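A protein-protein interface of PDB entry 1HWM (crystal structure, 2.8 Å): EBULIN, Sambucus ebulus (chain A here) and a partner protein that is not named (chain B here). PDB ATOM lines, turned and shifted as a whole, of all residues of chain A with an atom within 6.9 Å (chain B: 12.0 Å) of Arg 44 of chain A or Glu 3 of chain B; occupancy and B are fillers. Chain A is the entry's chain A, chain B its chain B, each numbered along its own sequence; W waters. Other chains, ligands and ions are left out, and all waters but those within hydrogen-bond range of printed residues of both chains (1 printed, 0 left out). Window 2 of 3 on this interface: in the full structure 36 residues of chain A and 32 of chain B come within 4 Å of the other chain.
NH2 of Arg 44 of chain A is in salt-bridge range of OE1 of Glu 3 of chain B (2.8 Å). The side-chain sulfur (SG) of Cys 5 of chain B is disulfide-bonded to the side-chain sulfur (SG) of Cys 249 of chain A, at 2.0 Å. SG of Cys 5 of chain B lies within hydrogen-bond range of N of Ala 251 of chain A (3.3 Å).
Among the printed residues, merely in contact across the chains: Val 250 of chain A with Thr 4 of chain B, Val 250 of chain A with Glu 3 of chain B and Val 250 of chain A with Cys 5 of chain B.
Arg 43 of chain A touches none of the printed residues of chain B. Arg 44 of chain A touches one residue of chain B. No residue of chain B comes within 4 Å of Glu 45 of chain A. No residue of chain B comes within 4 Å of Ser 46 of chain A. No residue of chain B comes within 4 Å of Glu 47 of chain A. Arg 53 of chain A touches none of the printed residues of chain B. No residue of chain B comes within 4 Å of Thr 74 of chain A. Cys 249 of chain A touches just one residue of chain B: Cys 5. Val 250 of chain A touches three residues of chain B. Of the printed residues of chain B, Ala 251 of chain A touches Cys 5. Glu 3 of chain B touches two residues of chain A. Printed residues of chain A within 4 Å of Thr 4 of chain B: Val 250. Of the printed residues of chain A, Cys 5 of chain B touches Cys 249, Val 250 and Ala 251. The nearest residue of chain B that does not touch Arg 44 of chain A is Thr 4 of chain B (6.8 Å).
Along chain A the printed residues that touch a printed residue of chain B span positions 44 to 251. Along chain B the printed residues that touch a printed residue of chain A span positions 3 to 5. Among the printed residues, Asp or Glu carboxylates within 4 Å of a Lys or Arg side-chain nitrogen of the other chain: Arg 44 of chain A with Glu 3 of chain B.
Water W1 lies within hydrogen-bond range of the backbone carbonyl oxygen of Cys 5 of chain B and the backbone carbonyl oxygen of Ala 251 of chain A.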
ATOM      1  N   VAL A  41      17.444 -18.164 -25.341  1.00  0.00           N
ATOM      2  CA  VAL A  41      16.050 -18.510 -25.604  1.00  0.00           C
ATOM      3  C   VAL A  41      15.663 -19.787 -24.862  1.00  0.00           C
ATOM      4  O   VAL A  41      16.122 -20.876 -25.206  1.00  0.00           O
ATOM      5  CB  VAL A  41      15.803 -18.725 -27.116  1.00  0.00           C
ATOM      6  CG1 VAL A  41      14.446 -19.371 -27.339  1.00  0.00           C
ATOM      7  CG2 VAL A  41      15.884 -17.399 -27.847  1.00  0.00           C
ATOM      8  N   LEU A  42      14.814 -19.652 -23.848  1.00  0.00           N
ATOM      9  CA  LEU A  42      14.370 -20.799 -23.062  1.00  0.00           C
ATOM     10  C   LEU A  42      14.103 -22.014 -23.946  1.00  0.00           C
ATOM     11  O   LEU A  42      13.425 -21.915 -24.968  1.00  0.00           O
ATOM     12  CB  LEU A  42      13.106 -20.442 -22.275  1.00  0.00           C
ATOM     13  CG  LEU A  42      13.219 -19.243 -21.331  1.00  0.00           C
ATOM     14  CD1 LEU A  42      11.917 -19.058 -20.575  1.00  0.00           C
ATOM     15  CD2 LEU A  42      14.367 -19.463 -20.363  1.00  0.00           C
ATOM     16  N   ARG A  43      14.643 -23.159 -23.543  1.00  0.00           N
ATOM     17  CA  ARG A  43      14.477 -24.392 -24.302  1.00  0.00           C
ATOM     18  C   ARG A  43      13.015 -24.668 -24.627  1.00  0.00           C
ATOM     19  O   ARG A  43      12.130 -24.425 -23.807  1.00  0.00           O
ATOM     20  CB  ARG A  43      15.047 -25.575 -23.517  1.00  0.00           C
ATOM     21  CG  ARG A  43      16.378 -25.300 -22.838  1.00  0.00           C
ATOM     22  CD  ARG A  43      17.232 -26.559 -22.792  1.00  0.00           C
ATOM     23  NE  ARG A  43      17.764 -26.826 -21.454  1.00  0.00           N
ATOM     24  CZ  ARG A  43      18.215 -28.013 -21.054  1.00  0.00           C
ATOM     25  NH1 ARG A  43      18.200 -29.047 -21.883  1.00  0.00           N
ATOM     26  NH2 ARG A  43      18.681 -28.167 -19.821  1.00  0.00           N
ATOM     27  N   ARG A  44      12.768 -25.171 -25.833  1.00  0.00           N
ATOM     28  CA  ARG A  44      11.412 -25.500 -26.262  1.00  0.00           C
ATOM     29  C   ARG A  44      10.874 -26.583 -25.334  1.00  0.00           C
ATOM     30  O   ARG A  44      11.646 -27.227 -24.623  1.00  0.00           O
ATOM     31  CB  ARG A  44      11.430 -26.025 -27.697  1.00  0.00           C
ATOM     32  CG  ARG A  44      11.157 -24.975 -28.756  1.00  0.00           C
ATOM     33  CD  ARG A  44      10.011 -25.407 -29.653  1.00  0.00           C
ATOM     34  NE  ARG A  44      10.431 -25.602 -31.040  1.00  0.00           N
ATOM     35  CZ  ARG A  44      11.296 -26.529 -31.439  1.00  0.00           C
ATOM     36  NH1 ARG A  44      11.842 -27.356 -30.556  1.00  0.00           N
ATOM     37  NH2 ARG A  44      11.608 -26.639 -32.724  1.00  0.00           N
ATOM     38  N   GLU A  45       9.559 -26.789 -25.329  1.00  0.00           N
ATOM     39  CA  GLU A  45       8.984 -27.826 -24.475  1.00  0.00           C
ATOM     40  C   GLU A  45       9.516 -29.177 -24.940  1.00  0.00           C
ATOM     41  O   GLU A  45       9.975 -29.987 -24.134  1.00  0.00           O
ATOM     42  CB  GLU A  45       7.452 -27.832 -24.554  1.00  0.00           C
ATOM     43  CG  GLU A  45       6.818 -29.144 -24.075  1.00  0.00           C
ATOM     44  CD  GLU A  45       5.295 -29.149 -24.185  1.00  0.00           C
ATOM     45  OE1 GLU A  45       4.645 -28.309 -23.523  1.00  0.00           O
ATOM     46  OE2 GLU A  45       4.750 -29.993 -24.932  1.00  0.00           O
ATOM     47  N   SER A  46       9.455 -29.406 -26.249  1.00  0.00           N
ATOM     48  CA  SER A  46       9.921 -30.653 -26.846  1.00  0.00           C
ATOM     49  C   SER A  46      11.440 -30.680 -26.970  1.00  0.00           C
ATOM     50  O   SER A  46      11.976 -30.728 -28.075  1.00  0.00           O
ATOM     51  CB  SER A  46       9.294 -30.837 -28.229  1.00  0.00           C
ATOM     52  OG  SER A  46       9.064 -29.584 -28.851  1.00  0.00           O
ATOM     53  N   GLU A  47      12.127 -30.653 -25.833  1.00  0.00           N
ATOM     54  CA  GLU A  47      13.586 -30.680 -25.805  1.00  0.00           C
ATOM     55  C   GLU A  47      14.071 -30.857 -24.370  1.00  0.00           C
ATOM     56  O   GLU A  47      15.130 -31.434 -24.122  1.00  0.00           O
ATOM     57  CB  GLU A  47      14.161 -29.383 -26.399  1.00  0.00           C
ATOM     58  CG  GLU A  47      14.684 -28.374 -25.372  1.00  0.00           C
ATOM     59  CD  GLU A  47      16.197 -28.194 -25.430  1.00  0.00           C
ATOM     60  OE1 GLU A  47      16.663 -27.324 -26.199  1.00  0.00           O
ATOM     61  OE2 GLU A  47      16.915 -28.921 -24.706  1.00  0.00           O
ATOM     62  N   VAL A  48      13.281 -30.358 -23.427  1.00  0.00           N
ATOM     63  CA  VAL A  48      13.625 -30.448 -22.017  1.00  0.00           C
ATOM     64  C   VAL A  48      13.146 -31.749 -21.379  1.00  0.00           C
ATOM     65  O   VAL A  48      11.947 -31.966 -21.217  1.00  0.00           O
ATOM     66  CB  VAL A  48      13.026 -29.261 -21.231  1.00  0.00           C
ATOM     67  CG1 VAL A  48      13.389 -29.371 -19.763  1.00  0.00           C
ATOM     68  CG2 VAL A  48      13.531 -27.947 -21.808  1.00  0.00           C
ATOM     69  N   ARG A  53      13.160 -29.945 -16.127  1.00  0.00           N
ATOM     70  CA  ARG A  53      12.113 -29.056 -16.621  1.00  0.00           C
ATOM     71  C   ARG A  53      11.746 -27.984 -15.605  1.00  0.00           C
ATOM     72  O   ARG A  53      11.363 -26.874 -15.975  1.00  0.00           O
ATOM     73  CB  ARG A  53      10.865 -29.865 -16.983  1.00  0.00           C
ATOM     74  CG  ARG A  53       9.635 -29.020 -17.285  1.00  0.00           C
ATOM     75  CD  ARG A  53       9.825 -28.200 -18.553  1.00  0.00           C
ATOM     76  NE  ARG A  53       8.565 -27.663 -19.064  1.00  0.00           N
ATOM     77  CZ  ARG A  53       7.571 -28.407 -19.532  1.00  0.00           C
ATOM     78  NH1 ARG A  53       7.687 -29.728 -19.556  1.00  0.00           N
ATOM     79  NH2 ARG A  53       6.463 -27.832 -19.977  1.00  0.00           N
ATOM     80  N   THR A  74      11.054 -23.812 -19.307  1.00  0.00           N
ATOM     81  CA  THR A  74      10.737 -23.480 -20.696  1.00  0.00           C
ATOM     82  C   THR A  74      10.127 -22.100 -20.915  1.00  0.00           C
ATOM     83  O   THR A  74      10.260 -21.527 -21.997  1.00  0.00           O
ATOM     84  CB  THR A  74       9.785 -24.521 -21.310  1.00  0.00           C
ATOM     85  OG1 THR A  74       8.497 -24.413 -20.694  1.00  0.00           O
ATOM     86  CG2 THR A  74      10.333 -25.923 -21.106  1.00  0.00           C
ATOM     87  N   PHE A 247      11.097 -18.665 -26.405  1.00  0.00           N
ATOM     88  CA  PHE A 247      11.033 -19.276 -27.723  1.00  0.00           C
ATOM     89  C   PHE A 247       9.649 -19.080 -28.333  1.00  0.00           C
ATOM     90  O   PHE A 247       8.636 -19.416 -27.723  1.00  0.00           O
ATOM     91  CB  PHE A 247      11.356 -20.770 -27.639  1.00  0.00           C
ATOM     92  CG  PHE A 247      11.363 -21.461 -28.972  1.00  0.00           C
ATOM     93  CD1 PHE A 247      12.564 -21.790 -29.594  1.00  0.00           C
ATOM     94  CD2 PHE A 247      10.170 -21.779 -29.613  1.00  0.00           C
ATOM     95  CE1 PHE A 247      12.575 -22.424 -30.831  1.00  0.00           C
ATOM     96  CE2 PHE A 247      10.171 -22.412 -30.849  1.00  0.00           C
ATOM     97  CZ  PHE A 247      11.377 -22.736 -31.458  1.00  0.00           C
ATOM     98  N   ARG A 248       9.619 -18.532 -29.541  1.00  0.00           N
ATOM     99  CA  ARG A 248       8.370 -18.293 -30.254  1.00  0.00           C
ATOM    100  C   ARG A 248       8.628 -18.621 -31.715  1.00  0.00           C
ATOM    101  O   ARG A 248       7.867 -19.341 -32.361  1.00  0.00           O
ATOM    102  CB  ARG A 248       7.955 -16.827 -30.117  1.00  0.00           C
ATOM    103  CG  ARG A 248       7.397 -16.470 -28.752  1.00  0.00           C
ATOM    104  CD  ARG A 248       6.013 -17.067 -28.553  1.00  0.00           C
ATOM    105  NE  ARG A 248       5.107 -16.721 -29.644  1.00  0.00           N
ATOM    106  CZ  ARG A 248       4.779 -15.476 -29.976  1.00  0.00           C
ATOM    107  NH1 ARG A 248       5.285 -14.450 -29.304  1.00  0.00           N
ATOM    108  NH2 ARG A 248       3.941 -15.254 -30.981  1.00  0.00           N
ATOM    109  N   CYS A 249       9.723 -18.072 -32.221  1.00  0.00           N
ATOM    110  CA  CYS A 249      10.138 -18.293 -33.594  1.00  0.00           C
ATOM    111  C   CYS A 249      11.201 -19.384 -33.607  1.00  0.00           C
ATOM    112  O   CYS A 249      11.325 -20.148 -32.652  1.00  0.00           O
ATOM    113  CB  CYS A 249      10.715 -17.000 -34.160  1.00  0.00           C
ATOM    114  SG  CYS A 249      10.269 -16.654 -35.884  1.00  0.00           S
ATOM    115  N   VAL A 250      11.959 -19.457 -34.695  1.00  0.00           N
ATOM    116  CA  VAL A 250      13.031 -20.440 -34.834  1.00  0.00           C
ATOM    117  C   VAL A 250      14.114 -19.825 -35.715  1.00  0.00           C
ATOM    118  O   VAL A 250      15.282 -20.214 -35.662  1.00  0.00           O
ATOM    119  CB  VAL A 250      12.531 -21.743 -35.505  1.00  0.00           C
ATOM    120  CG1 VAL A 250      13.695 -22.712 -35.700  1.00  0.00           C
ATOM    121  CG2 VAL A 250      11.443 -22.383 -34.659  1.00  0.00           C
ATOM    122  N   ALA A 251      13.703 -18.852 -36.521  1.00  0.00           N
ATOM    123  CA  ALA A 251      14.603 -18.156 -37.428  1.00  0.00           C
ATOM    124  C   ALA A 251      15.295 -19.129 -38.374  1.00  0.00           C
ATOM    125  O   ALA A 251      14.612 -19.625 -39.298  1.00  0.00           O
ATOM    126  CB  ALA A 251      15.634 -17.364 -36.631  1.00  0.00           C
ATOM    127  N   GLU B   3       7.866 -22.780 -35.344  1.00  0.00           N
ATOM    128  CA  GLU B   3       8.947 -23.315 -36.223  1.00  0.00           C
ATOM    129  C   GLU B   3       9.211 -22.430 -37.439  1.00  0.00           C
ATOM    130  O   GLU B   3       8.283 -21.993 -38.121  1.00  0.00           O
ATOM    131  CB  GLU B   3       8.600 -24.729 -36.694  1.00  0.00           C
ATOM    132  CG  GLU B   3       9.805 -25.647 -36.822  1.00  0.00           C
ATOM    133  CD  GLU B   3      10.103 -26.402 -35.534  1.00  0.00           C
ATOM    134  OE1 GLU B   3       9.547 -26.023 -34.478  1.00  0.00           O
ATOM    135  OE2 GLU B   3      10.890 -27.373 -35.580  1.00  0.00           O
ATOM    136  N   THR B   4      10.490 -22.185 -37.707  1.00  0.00           N
ATOM    137  CA  THR B   4      10.908 -21.355 -38.830  1.00  0.00           C
ATOM    138  C   THR B   4      10.310 -19.955 -38.795  1.00  0.00           C
ATOM    139  O   THR B   4       9.093 -19.780 -38.871  1.00  0.00           O
ATOM    140  CB  THR B   4      10.531 -22.009 -40.166  1.00  0.00           C
ATOM    141  OG1 THR B   4      11.112 -23.318 -40.232  1.00  0.00           O
ATOM    142  CG2 THR B   4      11.045 -21.171 -41.327  1.00  0.00           C
ATOM    143  N   CYS B   5      11.180 -18.956 -38.693  1.00  0.00           N
ATOM    144  CA  CYS B   5      10.747 -17.567 -38.639  1.00  0.00           C
ATOM    145  C   CYS B   5      10.021 -17.108 -39.893  1.00  0.00           C
ATOM    146  O   CYS B   5      10.565 -17.164 -40.996  1.00  0.00           O
ATOM    147  CB  CYS B   5      11.944 -16.652 -38.391  1.00  0.00           C
ATOM    148  SG  CYS B   5      12.025 -16.030 -36.686  1.00  0.00           S
ATOM    149  N   ALA B   6       8.786 -16.655 -39.714  1.00  0.00           N
ATOM    150  CA  ALA B   6       7.991 -16.164 -40.830  1.00  0.00           C
ATOM    151  C   ALA B   6       8.707 -14.985 -41.485  1.00  0.00           C
ATOM    152  O   ALA B   6       9.331 -14.169 -40.804  1.00  0.00           O
ATOM    153  CB  ALA B   6       6.609 -15.737 -40.342  1.00  0.00           C
ATOM    154  N   ILE B   7       8.621 -14.909 -42.809  1.00  0.00           N
ATOM    155  CA  ILE B   7       9.255 -13.826 -43.553  1.00  0.00           C
ATOM    156  C   ILE B   7       8.456 -12.550 -43.326  1.00  0.00           C
ATOM    157  O   ILE B   7       7.249 -12.511 -43.566  1.00  0.00           O
ATOM    158  CB  ILE B   7       9.302 -14.126 -45.067  1.00  0.00           C
ATOM    159  CG1 ILE B   7       8.079 -14.946 -45.478  1.00  0.00           C
ATOM    160  CG2 ILE B   7      10.581 -14.869 -45.408  1.00  0.00           C
ATOM    161  CD1 ILE B   7       6.908 -14.108 -45.955  1.00  0.00           C
ATOM    162  N   PRO B   8       9.123 -11.486 -42.858  1.00  0.00           N
ATOM    163  CA  PRO B   8       8.440 -10.216 -42.605  1.00  0.00           C
ATOM    164  C   PRO B   8       8.184  -9.410 -43.871  1.00  0.00           C
ATOM    165  O   PRO B   8       8.872  -9.573 -44.877  1.00  0.00           O
ATOM    166  CB  PRO B   8       9.384  -9.492 -41.653  1.00  0.00           C
ATOM    167  CG  PRO B   8      10.737  -9.999 -42.030  1.00  0.00           C
ATOM    168  CD  PRO B   8      10.561 -11.409 -42.547  1.00  0.00           C
HETATM  169  O   HOH W   1      13.454 -17.295 -41.355  1.00  0.00           O
